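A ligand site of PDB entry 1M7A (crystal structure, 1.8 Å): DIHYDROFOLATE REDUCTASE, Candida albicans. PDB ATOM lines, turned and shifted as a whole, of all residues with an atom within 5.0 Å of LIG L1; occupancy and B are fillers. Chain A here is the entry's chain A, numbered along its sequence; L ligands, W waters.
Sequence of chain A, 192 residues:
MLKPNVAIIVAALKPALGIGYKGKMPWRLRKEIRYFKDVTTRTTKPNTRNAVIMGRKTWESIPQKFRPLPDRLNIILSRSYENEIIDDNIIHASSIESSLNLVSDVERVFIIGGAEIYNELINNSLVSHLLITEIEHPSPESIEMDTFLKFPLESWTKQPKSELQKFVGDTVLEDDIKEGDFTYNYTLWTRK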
ATOM      1  N   VAL A  10       7.874  14.112 -35.934  1.00  0.00           N
ATOM      2  CA  VAL A  10       6.787  15.110 -35.920  1.00  0.00           C
ATOM      3  C   VAL A  10       5.879  14.981 -37.162  1.00  0.00           C
ATOM      4  O   VAL A  10       6.350  14.409 -38.171  1.00  0.00           O
ATOM      5  CB  VAL A  10       7.483  16.516 -35.900  1.00  0.00           C
ATOM      6  CG1 VAL A  10       8.390  16.740 -37.134  1.00  0.00           C
ATOM      7  CG2 VAL A  10       6.481  17.661 -35.829  1.00  0.00           C
ATOM      8  N   ALA A  11       4.653  15.460 -37.031  1.00  0.00           N
ATOM      9  CA  ALA A  11       3.699  15.479 -38.195  1.00  0.00           C
ATOM     10  C   ALA A  11       3.431  16.964 -38.496  1.00  0.00           C
ATOM     11  O   ALA A  11       3.100  17.759 -37.601  1.00  0.00           O
ATOM     12  CB  ALA A  11       2.417  14.748 -37.901  1.00  0.00           C
ATOM     13  N   ILE A  19       2.014  22.745 -36.882  1.00  0.00           N
ATOM     14  CA  ILE A  19       1.950  21.610 -35.998  1.00  0.00           C
ATOM     15  C   ILE A  19       0.924  21.648 -34.884  1.00  0.00           C
ATOM     16  O   ILE A  19       0.750  20.602 -34.208  1.00  0.00           O
ATOM     17  CB  ILE A  19       3.363  21.201 -35.403  1.00  0.00           C
ATOM     18  CG1 ILE A  19       3.910  22.295 -34.446  1.00  0.00           C
ATOM     19  CG2 ILE A  19       4.376  20.910 -36.568  1.00  0.00           C
ATOM     20  CD1 ILE A  19       5.221  21.984 -33.717  1.00  0.00           C
ATOM     21  N   GLY A  20       0.296  22.814 -34.616  1.00  0.00           N
ATOM     22  CA  GLY A  20      -0.689  22.808 -33.518  1.00  0.00           C
ATOM     23  C   GLY A  20      -1.518  24.079 -33.513  1.00  0.00           C
ATOM     24  O   GLY A  20      -1.207  25.077 -34.163  1.00  0.00           O
ATOM     25  N   TYR A  21      -2.477  24.024 -32.601  1.00  0.00           N
ATOM     26  CA  TYR A  21      -3.400  25.160 -32.422  1.00  0.00           C
ATOM     27  C   TYR A  21      -4.047  25.036 -31.046  1.00  0.00           C
ATOM     28  O   TYR A  21      -4.705  24.048 -30.720  1.00  0.00           O
ATOM     29  CB  TYR A  21      -4.472  25.146 -33.504  1.00  0.00           C
ATOM     30  CG  TYR A  21      -5.465  26.284 -33.421  1.00  0.00           C
ATOM     31  CD1 TYR A  21      -6.748  26.075 -32.892  1.00  0.00           C
ATOM     32  CD2 TYR A  21      -5.103  27.567 -33.831  1.00  0.00           C
ATOM     33  CE1 TYR A  21      -7.669  27.132 -32.838  1.00  0.00           C
ATOM     34  CE2 TYR A  21      -5.998  28.623 -33.767  1.00  0.00           C
ATOM     35  CZ  TYR A  21      -7.281  28.402 -33.260  1.00  0.00           C
ATOM     36  OH  TYR A  21      -8.129  29.471 -33.218  1.00  0.00           O
ATOM     37  N   GLY A  23      -2.802  24.519 -28.049  1.00  0.00           N
ATOM     38  CA  GLY A  23      -2.284  23.406 -27.273  1.00  0.00           C
ATOM     39  C   GLY A  23      -2.667  22.036 -27.751  1.00  0.00           C
ATOM     40  O   GLY A  23      -2.323  21.050 -27.064  1.00  0.00           O
ATOM     41  N   LYS A  24      -3.337  21.931 -28.894  1.00  0.00           N
ATOM     42  CA  LYS A  24      -3.774  20.655 -29.446  1.00  0.00           C
ATOM     43  C   LYS A  24      -3.292  20.440 -30.873  1.00  0.00           C
ATOM     44  O   LYS A  24      -2.901  21.374 -31.588  1.00  0.00           O
ATOM     45  CB  LYS A  24      -5.265  20.421 -29.336  1.00  0.00           C
ATOM     46  CG  LYS A  24      -6.315  21.264 -29.958  1.00  0.00           C
ATOM     47  CD  LYS A  24      -6.267  21.545 -31.417  1.00  0.00           C
ATOM     48  CE  LYS A  24      -7.222  22.399 -32.147  1.00  0.00           C
ATOM     49  NZ  LYS A  24      -8.104  21.570 -33.055  1.00  0.00           N
ATOM     50  N   MET A  25      -3.461  19.190 -31.324  1.00  0.00           N
ATOM     51  CA  MET A  25      -3.146  18.874 -32.757  1.00  0.00           C
ATOM     52  C   MET A  25      -4.400  19.257 -33.578  1.00  0.00           C
ATOM     53  O   MET A  25      -5.531  19.003 -33.162  1.00  0.00           O
ATOM     54  CB  MET A  25      -2.663  17.475 -32.960  1.00  0.00           C
ATOM     55  CG  MET A  25      -1.331  17.233 -32.289  1.00  0.00           C
ATOM     56  SD  MET A  25      -0.903  15.480 -32.519  1.00  0.00           S
ATOM     57  CE  MET A  25      -0.327  15.572 -34.258  1.00  0.00           C
ATOM     58  N   TRP A  27      -5.636  18.138 -36.267  1.00  0.00           N
ATOM     59  CA  TRP A  27      -6.134  16.994 -37.027  1.00  0.00           C
ATOM     60  C   TRP A  27      -6.133  15.778 -36.135  1.00  0.00           C
ATOM     61  O   TRP A  27      -5.532  15.716 -35.030  1.00  0.00           O
ATOM     62  CB  TRP A  27      -5.247  16.734 -38.291  1.00  0.00           C
ATOM     63  CG  TRP A  27      -3.769  16.680 -37.959  1.00  0.00           C
ATOM     64  CD1 TRP A  27      -3.048  15.737 -37.295  1.00  0.00           C
ATOM     65  CD2 TRP A  27      -2.839  17.738 -38.284  1.00  0.00           C
ATOM     66  NE1 TRP A  27      -1.734  16.131 -37.177  1.00  0.00           N
ATOM     67  CE2 TRP A  27      -1.582  17.350 -37.771  1.00  0.00           C
ATOM     68  CE3 TRP A  27      -2.983  18.982 -38.872  1.00  0.00           C
ATOM     69  CZ2 TRP A  27      -0.464  18.161 -37.891  1.00  0.00           C
ATOM     70  CZ3 TRP A  27      -1.862  19.788 -39.022  1.00  0.00           C
ATOM     71  CH2 TRP A  27      -0.633  19.385 -38.519  1.00  0.00           C
ATOM     72  N   GLY A  55       8.486  17.865 -23.895  1.00  0.00           N
ATOM     73  CA  GLY A  55       8.385  19.058 -23.009  1.00  0.00           C
ATOM     74  C   GLY A  55       7.225  18.837 -22.005  1.00  0.00           C
ATOM     75  O   GLY A  55       6.368  17.976 -22.165  1.00  0.00           O
ATOM     76  N   ARG A  56       7.262  19.549 -20.901  1.00  0.00           N
ATOM     77  CA  ARG A  56       6.257  19.411 -19.805  1.00  0.00           C
ATOM     78  C   ARG A  56       4.840  19.645 -20.334  1.00  0.00           C
ATOM     79  O   ARG A  56       3.884  18.952 -19.891  1.00  0.00           O
ATOM     80  CB  ARG A  56       6.561  20.366 -18.663  1.00  0.00           C
ATOM     81  CG  ARG A  56       5.641  20.171 -17.425  1.00  0.00           C
ATOM     82  CD  ARG A  56       5.893  21.178 -16.373  1.00  0.00           C
ATOM     83  NE  ARG A  56       5.861  22.581 -16.737  1.00  0.00           N
ATOM     84  CZ  ARG A  56       4.941  23.396 -17.187  1.00  0.00           C
ATOM     85  NH1 ARG A  56       5.226  24.591 -17.739  1.00  0.00           N
ATOM     86  NH2 ARG A  56       3.640  23.119 -17.131  1.00  0.00           N
ATOM     87  N   LYS A  57       4.698  20.636 -21.233  1.00  0.00           N
ATOM     88  CA  LYS A  57       3.356  20.939 -21.743  1.00  0.00           C
ATOM     89  C   LYS A  57       2.757  19.810 -22.550  1.00  0.00           C
ATOM     90  O   LYS A  57       1.530  19.531 -22.448  1.00  0.00           O
ATOM     91  CB  LYS A  57       3.298  22.239 -22.543  1.00  0.00           C
ATOM     92  CG  LYS A  57       3.725  23.444 -21.662  1.00  0.00           C
ATOM     93  CD  LYS A  57       3.712  24.668 -22.581  1.00  0.00           C
ATOM     94  CE  LYS A  57       3.880  25.974 -21.833  1.00  0.00           C
ATOM     95  NZ  LYS A  57       5.114  25.975 -21.022  1.00  0.00           N
ATOM     96  N   THR A  58       3.544  19.107 -23.342  1.00  0.00           N
ATOM     97  CA  THR A  58       3.057  17.927 -24.098  1.00  0.00           C
ATOM     98  C   THR A  58       2.664  16.807 -23.124  1.00  0.00           C
ATOM     99  O   THR A  58       1.614  16.177 -23.315  1.00  0.00           O
ATOM    100  CB  THR A  58       4.019  17.461 -25.232  1.00  0.00           C
ATOM    101  OG1 THR A  58       4.036  18.590 -26.194  1.00  0.00           O
ATOM    102  CG2 THR A  58       3.533  16.219 -26.047  1.00  0.00           C
ATOM    103  N   LEU A  77      11.009  17.038 -19.862  1.00  0.00           N
ATOM    104  CA  LEU A  77      11.902  18.165 -19.590  1.00  0.00           C
ATOM    105  C   LEU A  77      11.099  19.370 -19.091  1.00  0.00           C
ATOM    106  O   LEU A  77      10.106  19.824 -19.702  1.00  0.00           O
ATOM    107  CB  LEU A  77      12.648  18.527 -20.887  1.00  0.00           C
ATOM    108  CG  LEU A  77      13.517  17.584 -21.638  1.00  0.00           C
ATOM    109  CD1 LEU A  77      14.224  18.316 -22.777  1.00  0.00           C
ATOM    110  CD2 LEU A  77      14.508  16.829 -20.816  1.00  0.00           C
ATOM    111  N   SER A  78      11.719  19.969 -18.050  1.00  0.00           N
ATOM    112  CA  SER A  78      11.191  21.212 -17.465  1.00  0.00           C
ATOM    113  C   SER A  78      12.491  21.915 -16.931  1.00  0.00           C
ATOM    114  O   SER A  78      13.358  21.189 -16.397  1.00  0.00           O
ATOM    115  CB  SER A  78      10.245  20.975 -16.311  1.00  0.00           C
ATOM    116  OG  SER A  78       9.947  22.201 -15.634  1.00  0.00           O
ATOM    117  N   ARG A  79      12.527  23.197 -17.103  1.00  0.00           N
ATOM    118  CA  ARG A  79      13.671  23.995 -16.554  1.00  0.00           C
ATOM    119  C   ARG A  79      13.647  24.023 -15.023  1.00  0.00           C
ATOM    120  O   ARG A  79      14.676  24.300 -14.361  1.00  0.00           O
ATOM    121  CB  ARG A  79      13.672  25.390 -17.189  1.00  0.00           C
ATOM    122  CG  ARG A  79      14.082  25.351 -18.661  1.00  0.00           C
ATOM    123  CD  ARG A  79      14.097  26.732 -19.234  1.00  0.00           C
ATOM    124  NE  ARG A  79      14.011  26.793 -20.694  1.00  0.00           N
ATOM    125  CZ  ARG A  79      12.896  26.895 -21.413  1.00  0.00           C
ATOM    126  NH1 ARG A  79      11.685  27.085 -20.895  1.00  0.00           N
ATOM    127  NH2 ARG A  79      13.003  26.780 -22.747  1.00  0.00           N
ATOM    128  N   SER A  80      12.538  23.675 -14.427  1.00  0.00           N
ATOM    129  CA  SER A  80      12.396  23.622 -12.943  1.00  0.00           C
ATOM    130  C   SER A  80      12.650  22.247 -12.378  1.00  0.00           C
ATOM    131  O   SER A  80      12.470  22.017 -11.139  1.00  0.00           O
ATOM    132  CB  SER A  80      11.072  24.148 -12.501  1.00  0.00           C
ATOM    133  OG  SER A  80      10.626  25.374 -12.919  1.00  0.00           O
ATOM    134  N   SER A  94      16.267  18.495 -16.743  1.00  0.00           N
ATOM    135  CA  SER A  94      16.238  19.859 -17.201  1.00  0.00           C
ATOM    136  C   SER A  94      16.996  20.041 -18.535  1.00  0.00           C
ATOM    137  O   SER A  94      17.041  21.196 -18.985  1.00  0.00           O
ATOM    138  CB  SER A  94      16.664  20.887 -16.162  1.00  0.00           C
ATOM    139  OG  SER A  94      17.984  20.554 -15.765  1.00  0.00           O
ATOM    140  N   SER A  95      17.629  18.996 -19.029  1.00  0.00           N
ATOM    141  CA  SER A  95      18.330  19.084 -20.315  1.00  0.00           C
ATOM    142  C   SER A  95      18.388  17.650 -20.910  1.00  0.00           C
ATOM    143  O   SER A  95      18.392  16.653 -20.211  1.00  0.00           O
ATOM    144  CB  SER A  95      19.745  19.633 -20.286  1.00  0.00           C
ATOM    145  OG  SER A  95      20.644  18.849 -19.608  1.00  0.00           O
ATOM    146  N   ILE A 112       9.697  13.792 -29.123  1.00  0.00           N
ATOM    147  CA  ILE A 112       8.297  13.750 -29.587  1.00  0.00           C
ATOM    148  C   ILE A 112       7.502  15.022 -29.473  1.00  0.00           C
ATOM    149  O   ILE A 112       6.270  14.985 -29.777  1.00  0.00           O
ATOM    150  CB  ILE A 112       7.569  12.472 -29.031  1.00  0.00           C
ATOM    151  CG1 ILE A 112       7.268  12.692 -27.519  1.00  0.00           C
ATOM    152  CG2 ILE A 112       8.379  11.187 -29.348  1.00  0.00           C
ATOM    153  CD1 ILE A 112       6.047  11.908 -26.957  1.00  0.00           C
ATOM    154  N   GLY A 113       8.082  16.140 -29.137  1.00  0.00           N
ATOM    155  CA  GLY A 113       7.352  17.425 -29.091  1.00  0.00           C
ATOM    156  C   GLY A 113       7.512  18.085 -27.744  1.00  0.00           C
ATOM    157  O   GLY A 113       8.114  17.517 -26.809  1.00  0.00           O
ATOM    158  N   GLY A 114       6.949  19.283 -27.556  1.00  0.00           N
ATOM    159  CA  GLY A 114       6.168  20.035 -28.512  1.00  0.00           C
ATOM    160  C   GLY A 114       7.008  21.086 -29.202  1.00  0.00           C
ATOM    161  O   GLY A 114       8.190  20.914 -29.400  1.00  0.00           O
ATOM    162  N   ALA A 115       6.320  22.160 -29.658  1.00  0.00           N
ATOM    163  CA  ALA A 115       7.023  23.174 -30.478  1.00  0.00           C
ATOM    164  C   ALA A 115       8.276  23.771 -29.926  1.00  0.00           C
ATOM    165  O   ALA A 115       9.304  23.862 -30.634  1.00  0.00           O
ATOM    166  CB  ALA A 115       6.046  24.298 -30.800  1.00  0.00           C
ATOM    167  N   GLU A 116       8.224  24.156 -28.670  1.00  0.00           N
ATOM    168  CA  GLU A 116       9.421  24.780 -28.044  1.00  0.00           C
ATOM    169  C   GLU A 116      10.560  23.812 -28.051  1.00  0.00           C
ATOM    170  O   GLU A 116      11.674  24.184 -28.453  1.00  0.00           O
ATOM    171  CB  GLU A 116       9.028  25.372 -26.717  1.00  0.00           C
ATOM    172  CG  GLU A 116      10.190  26.071 -25.982  1.00  0.00           C
ATOM    173  CD  GLU A 116       9.903  26.783 -24.704  1.00  0.00           C
ATOM    174  OE1 GLU A 116      10.816  27.344 -24.106  1.00  0.00           O
ATOM    175  OE2 GLU A 116       8.723  26.759 -24.321  1.00  0.00           O
ATOM    176  N   ILE A 117      10.323  22.575 -27.616  1.00  0.00           N
ATOM    177  CA  ILE A 117      11.358  21.507 -27.652  1.00  0.00           C
ATOM    178  C   ILE A 117      11.925  21.325 -29.056  1.00  0.00           C
ATOM    179  O   ILE A 117      13.161  21.195 -29.304  1.00  0.00           O
ATOM    180  CB  ILE A 117      10.700  20.199 -27.088  1.00  0.00           C
ATOM    181  CG1 ILE A 117      10.334  20.408 -25.587  1.00  0.00           C
ATOM    182  CG2 ILE A 117      11.571  18.936 -27.320  1.00  0.00           C
ATOM    183  CD1 ILE A 117      11.537  20.570 -24.614  1.00  0.00           C
ATOM    184  N   TYR A 118      11.025  21.160 -30.028  1.00  0.00           N
ATOM    185  CA  TYR A 118      11.471  20.977 -31.433  1.00  0.00           C
ATOM    186  C   TYR A 118      12.353  22.080 -31.999  1.00  0.00           C
ATOM    187  O   TYR A 118      13.429  21.804 -32.563  1.00  0.00           O
ATOM    188  CB  TYR A 118      10.261  20.861 -32.374  1.00  0.00           C
ATOM    189  CG  TYR A 118       9.416  19.611 -32.343  1.00  0.00           C
ATOM    190  CD1 TYR A 118       9.976  18.316 -32.326  1.00  0.00           C
ATOM    191  CD2 TYR A 118       8.044  19.740 -32.518  1.00  0.00           C
ATOM    192  CE1 TYR A 118       9.169  17.204 -32.361  1.00  0.00           C
ATOM    193  CE2 TYR A 118       7.221  18.623 -32.550  1.00  0.00           C
ATOM    194  CZ  TYR A 118       7.793  17.374 -32.533  1.00  0.00           C
ATOM    195  OH  TYR A 118       6.968  16.282 -32.614  1.00  0.00           O
ATOM    196  N   GLU A 120      14.044  24.326 -30.544  1.00  0.00           N
ATOM    197  CA  GLU A 120      15.329  24.528 -29.798  1.00  0.00           C
ATOM    198  C   GLU A 120      16.271  23.369 -30.052  1.00  0.00           C
ATOM    199  O   GLU A 120      17.442  23.595 -30.419  1.00  0.00           O
ATOM    200  CB  GLU A 120      15.053  24.567 -28.318  1.00  0.00           C
ATOM    201  CG  GLU A 120      15.692  25.509 -27.381  1.00  0.00           C
ATOM    202  CD  GLU A 120      14.802  26.574 -26.787  1.00  0.00           C
ATOM    203  OE1 GLU A 120      14.382  26.454 -25.627  1.00  0.00           O
ATOM    204  OE2 GLU A 120      14.610  27.508 -27.566  1.00  0.00           O
ATOM    205  N   LEU A 121      15.817  22.135 -29.926  1.00  0.00           N
ATOM    206  CA  LEU A 121      16.649  20.937 -30.100  1.00  0.00           C
ATOM    207  C   LEU A 121      17.054  20.595 -31.497  1.00  0.00           C
ATOM    208  O   LEU A 121      18.043  19.825 -31.716  1.00  0.00           O
ATOM    209  CB  LEU A 121      16.115  19.836 -29.189  1.00  0.00           C
ATOM    210  CG  LEU A 121      15.943  20.139 -27.715  1.00  0.00           C
ATOM    211  CD1 LEU A 121      15.176  19.046 -27.010  1.00  0.00           C
ATOM    212  CD2 LEU A 121      17.304  20.335 -27.032  1.00  0.00           C
ATOM    213  N   THR A 147       1.033  27.435 -34.190  1.00  0.00           N
ATOM    214  CA  THR A 147       2.372  26.915 -33.768  1.00  0.00           C
ATOM    215  C   THR A 147       3.048  26.266 -34.956  1.00  0.00           C
ATOM    216  O   THR A 147       2.373  25.452 -35.545  1.00  0.00           O
ATOM    217  CB  THR A 147       2.036  25.884 -32.621  1.00  0.00           C
ATOM    218  OG1 THR A 147       1.433  26.745 -31.572  1.00  0.00           O
ATOM    219  CG2 THR A 147       3.111  25.048 -32.103  1.00  0.00           C
HETATM  220  P1  LIG L   1       6.254  21.781 -25.132  1.00  0.00           P
HETATM  221  O1  LIG L   1       5.659  20.395 -25.132  1.00  0.00           O
HETATM  222  O2  LIG L   1       7.366  21.992 -26.071  1.00  0.00           O
HETATM  223  O3  LIG L   1       6.656  22.144 -23.635  1.00  0.00           O
HETATM  224  C1  LIG L   1       7.421  23.376 -23.381  1.00  0.00           C
HETATM  225  C2  LIG L   1       7.989  23.280 -21.957  1.00  0.00           C
HETATM  226  O4  LIG L   1       9.109  22.337 -21.967  1.00  0.00           O
HETATM  227  C3  LIG L   1       8.560  24.633 -21.459  1.00  0.00           C
HETATM  228  O5  LIG L   1       7.492  25.322 -20.751  1.00  0.00           O
HETATM  229  C4  LIG L   1       9.673  24.106 -20.462  1.00  0.00           C
HETATM  230  O6  LIG L   1       9.103  23.581 -19.251  1.00  0.00           O
HETATM  231  C5  LIG L   1      10.140  22.879 -21.223  1.00  0.00           C
HETATM  232  N1  LIG L   1      11.252  23.157 -22.045  1.00  0.00           N
HETATM  233  C6  LIG L   1      11.214  23.753 -23.277  1.00  0.00           C
HETATM  234  N2  LIG L   1      12.403  23.838 -23.810  1.00  0.00           N
HETATM  235  C7  LIG L   1      13.231  23.296 -22.847  1.00  0.00           C
HETATM  236  C8  LIG L   1      14.634  23.094 -22.874  1.00  0.00           C
HETATM  237  N3  LIG L   1      15.356  23.510 -23.913  1.00  0.00           N
HETATM  238  N4  LIG L   1      15.166  22.517 -21.778  1.00  0.00           N
HETATM  239  C9  LIG L   1      14.333  22.157 -20.732  1.00  0.00           C
HETATM  240  N5  LIG L   1      13.022  22.262 -20.631  1.00  0.00           N
HETATM  241  C10 LIG L   1      12.532  22.837 -21.777  1.00  0.00           C
HETATM  242  O7  LIG L   1       5.128  22.797 -25.470  1.00  0.00           O
HETATM  243  P2  LIG L   1       4.600  23.809 -26.607  1.00  0.00           P
HETATM  244  O8  LIG L   1       3.455  24.536 -25.985  1.00  0.00           O
HETATM  245  O9  LIG L   1       5.593  24.684 -27.242  1.00  0.00           O
HETATM  246  O10 LIG L   1       3.999  22.786 -27.682  1.00  0.00           O
HETATM  247  C11 LIG L   1       2.684  22.160 -27.536  1.00  0.00           C
HETATM  248  C12 LIG L   1       2.141  22.267 -29.021  1.00  0.00           C
HETATM  249  O11 LIG L   1       2.884  21.282 -29.767  1.00  0.00           O
HETATM  250  C13 LIG L   1       0.648  21.859 -29.111  1.00  0.00           C
HETATM  251  O12 LIG L   1       0.021  22.594 -30.157  1.00  0.00           O
HETATM  252  C14 LIG L   1       0.842  20.360 -29.401  1.00  0.00           C
HETATM  253  O13 LIG L   1      -0.373  19.762 -29.830  1.00  0.00           O
HETATM  254  C15 LIG L   1       1.978  20.373 -30.373  1.00  0.00           C
HETATM  255  N6  LIG L   1       2.639  19.083 -30.680  1.00  0.00           N
HETATM  256  C16 LIG L   1       2.548  18.713 -32.056  1.00  0.00           C
HETATM  257  C17 LIG L   1       3.056  17.514 -32.457  1.00  0.00           C
HETATM  258  C18 LIG L   1       2.967  17.101 -33.971  1.00  0.00           C
HETATM  259  O14 LIG L   1       3.557  16.114 -34.334  1.00  0.00           O
HETATM  260  N7  LIG L   1       2.267  17.918 -34.801  1.00  0.00           N
HETATM  261  C19 LIG L   1       3.742  16.546 -31.588  1.00  0.00           C
HETATM  262  C20 LIG L   1       3.720  17.043 -30.260  1.00  0.00           C
HETATM  263  C21 LIG L   1       3.217  18.199 -29.783  1.00  0.00           C
HETATM  264  P3  LIG L   1       8.878  24.612 -17.956  1.00  0.00           P
HETATM  265  O15 LIG L   1       8.339  23.607 -16.947  1.00  0.00           O
HETATM  266  O16 LIG L   1      10.285  25.017 -17.680  1.00  0.00           O
HETATM  267  O17 LIG L   1       8.035  25.693 -18.423  1.00  0.00           O
HETATM  268  C1  LG2 L   2      -0.091  12.784 -28.970  1.00  0.00           C
HETATM  269  C2  LG2 L   2       0.015  11.863 -27.740  1.00  0.00           C
HETATM  270  O1  LG2 L   2       0.132  10.597 -28.288  1.00  0.00           O
HETATM  271  C3  LG2 L   2       0.807   9.634 -27.567  1.00  0.00           C
HETATM  272  C4  LG2 L   2      -0.350  14.252 -28.599  1.00  0.00           C
HETATM  273  O2  LG2 L   2       0.003  14.413 -27.223  1.00  0.00           O
HETATM  274  C5  LG2 L   2      -1.142  14.818 -26.485  1.00  0.00           C
HETATM  275  N1  LG2 L   2       2.896  11.784 -34.825  1.00  0.00           N
HETATM  276  N2  LG2 L   2       5.026  12.590 -34.292  1.00  0.00           N
HETATM  277  N3  LG2 L   2       1.182  12.684 -29.631  1.00  0.00           N
HETATM  278  N4  LG2 L   2       4.560  11.749 -36.421  1.00  0.00           N
HETATM  279  N5  LG2 L   2       5.549  13.450 -32.229  1.00  0.00           N
HETATM  280  C6  LG2 L   2       2.428  11.977 -33.502  1.00  0.00           C
HETATM  281  C7  LG2 L   2       4.175  12.035 -35.151  1.00  0.00           C
HETATM  282  C8  LG2 L   2       4.630  12.871 -33.056  1.00  0.00           C
HETATM  283  C9  LG2 L   2       3.303  12.585 -32.552  1.00  0.00           C
HETATM  284  C10 LG2 L   2       2.799  12.753 -31.238  1.00  0.00           C
HETATM  285  C11 LG2 L   2       3.376  13.333 -29.990  1.00  0.00           C
HETATM  286  C12 LG2 L   2       2.289  13.236 -29.087  1.00  0.00           C
HETATM  287  C13 LG2 L   2       1.434  12.412 -30.966  1.00  0.00           C
HETATM  288  C14 LG2 L   2       0.624  11.839 -31.939  1.00  0.00           C
HETATM  289  C15 LG2 L   2       1.055  11.828 -33.221  1.00  0.00           C
HETATM  290  O   HOH W   1      10.529  27.727 -18.662  1.00  0.00           O
HETATM  291  O   HOH W   2       1.357  19.180 -26.649  1.00  0.00           O
HETATM  292  O   HOH W   3       5.880  26.999 -28.317  1.00  0.00           O
HETATM  293  O   HOH W   4      16.093  26.697 -22.669  1.00  0.00           O
HETATM  294  O   HOH W   5       7.482  24.889 -14.479  1.00  0.00           O
HETATM  295  O   HOH W   6      18.261  24.296 -24.087  1.00  0.00           O
HETATM  296  O   HOH W   7       3.359  26.928 -24.866  1.00  0.00           O
HETATM  297  O   HOH W   8       0.850  24.129 -25.042  1.00  0.00           O
HETATM  298  O   HOH W   9      -0.532  25.257 -29.506  1.00  0.00           O
HETATM  299  O   HOH W  10      -1.046  17.969 -27.425  1.00  0.00           O
HETATM  300  O   HOH W  11       8.288  28.009 -21.994  1.00  0.00           O
HETATM  301  O   HOH W  12       5.965  26.781 -24.949  1.00  0.00           O
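The backbone carbonyl oxygen (O) of Ile 19 is in hydrogen-bond range of a nitrogen (N7) of LIG L1 (3.1 Å). NE of Arg 56 lies within salt-bridge range of O15 of LIG L1. O10 of LIG L1 lies within hydrogen-bond range of N of Ala 115, at 3.1 Å. The backbone NH (N) of Ala 11 is in hydrogen-bond range of an oxygen (O14) of LIG L1. The backbone carbonyl oxygen of Ala 11 sits at hydrogen-bond distance from a nitrogen (N7) of LIG L1 (2.9 Å). The side-chain amino group (NZ) of Lys 57 lies within salt-bridge range of an oxygen (O17) of LIG L1 (3.9 Å). The side-chain hydroxyl (OH) of Tyr 118 sits at hydrogen-bond distance from a nitrogen (N5) of LG2 L2, 3.2 Å away. The side-chain hydroxyl (OG1) of Thr 58 sits at hydrogen-bond distance from an oxygen (O1) of LIG L1. N of Arg 79 sits at hydrogen-bond distance from O16 of LIG L1 (2.9 Å). The backbone carbonyl oxygen of Ile 112 sits at hydrogen-bond distance from a nitrogen (N5) of LG2 L2 (3.0 Å). The backbone NH (N) of Met 25 is in hydrogen-bond range of an oxygen (O13) of LIG L1, 3.5 Å away. The guanidinium group (NH2) of Arg 79 is in hydrogen-bond range of a nitrogen (N2) of LIG L1 (3.2 Å). An oxygen (O2) of LIG L1 sits at hydrogen-bond distance from the backbone NH (N) of Ile 117, 3.4 Å away. The backbone NH of Glu 116 is in hydrogen-bond range of an oxygen (O9) of LIG L1 (3.0 Å). The side-chain hydroxyl (OG) of Ser 78 is in hydrogen-bond range of an oxygen (O15) of LIG L1 (2.5 Å). N of Lys 57 lies within hydrogen-bond range of O3 of LIG L1 (3.4 Å). O1 of LIG L1 is in hydrogen-bond range of N of Gly 114. An oxygen (O1) of LIG L1 is in hydrogen-bond range of the backbone NH of Thr 58, at 3.1 Å. The backbone carbonyl oxygen (O) of Lys 24 is in hydrogen-bond range of an oxygen (O12) of LIG L1 (3.5 Å).
The backbone NH (N) of Gly 55 sits at hydrogen-bond distance from the backbone carbonyl oxygen (O) of Gly 113. The backbone NH (N) of Ile 19 is in hydrogen-bond range of the backbone carbonyl oxygen (O) of Thr 147, at 3.0 Å. The backbone carbonyl oxygen of Leu 77 lies within hydrogen-bond range of the backbone NH of Arg 56 (3.1 Å). N of Gly 114 is in hydrogen-bond range of OG1 of Thr 58 (3.3 Å). The backbone NH (N) of Thr 147 is in hydrogen-bond range of the backbone carbonyl oxygen (O) of Gly 20 (3.3 Å). O of Ile 112 sits at hydrogen-bond distance from OH of Tyr 118. The guanidinium group of Arg 79 is in salt-bridge range of the side-chain carboxylate of Glu 120, at 3.2 Å. N of Ser 80 sits close to OG of Ser 78, 3.2 Å away.
CG2 of Val 10 touches O14 of LIG L1, 3.6 Å away. CA of Gly 20 touches O12 of LIG L1, at 3.4 Å. Tyr 21 touches LIG L1 (N to O12, 3.8 Å). Gly 23 touches LIG L1 (C to C13, 3.6 Å). Gly 55 touches LIG L1. O of Leu 77 touches C5 of LIG L1, at 3.4 Å. Ser 94 touches LIG L1. Ile 112 touches LIG L1 (O to C20, 3.3 Å). Gly 113 touches LIG L1. OH of Tyr 118 touches C19 of LIG L1 (3.4 Å). Glu 120 touches LIG L1 (OE1 to N3, 3.5 Å). Within 4 Å of LIG L1: Val 10, Ala 11, Ile 19, Gly 20, Tyr 21, Gly 23, Lys 24, Met 25, Gly 55, Arg 56, Lys 57, Thr 58, Leu 77, Ser 78, Arg 79, Ser 94, Ile 112, Gly 113, Gly 114, Ala 115, Glu 116, Ile 117, Tyr 118 and Glu 120. The nearest printed residue that does not touch LIG L1 is Trp 27 (4.1 Å).
Water W9 lies within hydrogen-bond range of N of Gly 23 (2.8 Å), O12 of LIG L1 (2.8 Å) and OG1 of Thr 147 (3.2 Å). Water W1 bridges NH1 of Arg 79 and O16 of LIG L1. Water W11 bridges the side-chain carboxylate of Glu 116 and an oxygen (O5) of LIG L1. Water W10 lies within hydrogen-bond range of O13 of LIG L1 (3.1 Å) and O of Gly 23 (3.4 Å). Water W12 lies within hydrogen-bond range of the side-chain carboxylate (OE2) of Glu 116 (2.8 Å) and an oxygen (O9) of LIG L1 (3.1 Å). Water W4 lies within hydrogen-bond range of NE of Arg 79 (2.9 Å), OE1 of Glu 120 (3.4 Å) and N3 of LIG L1 (3.5 Å).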
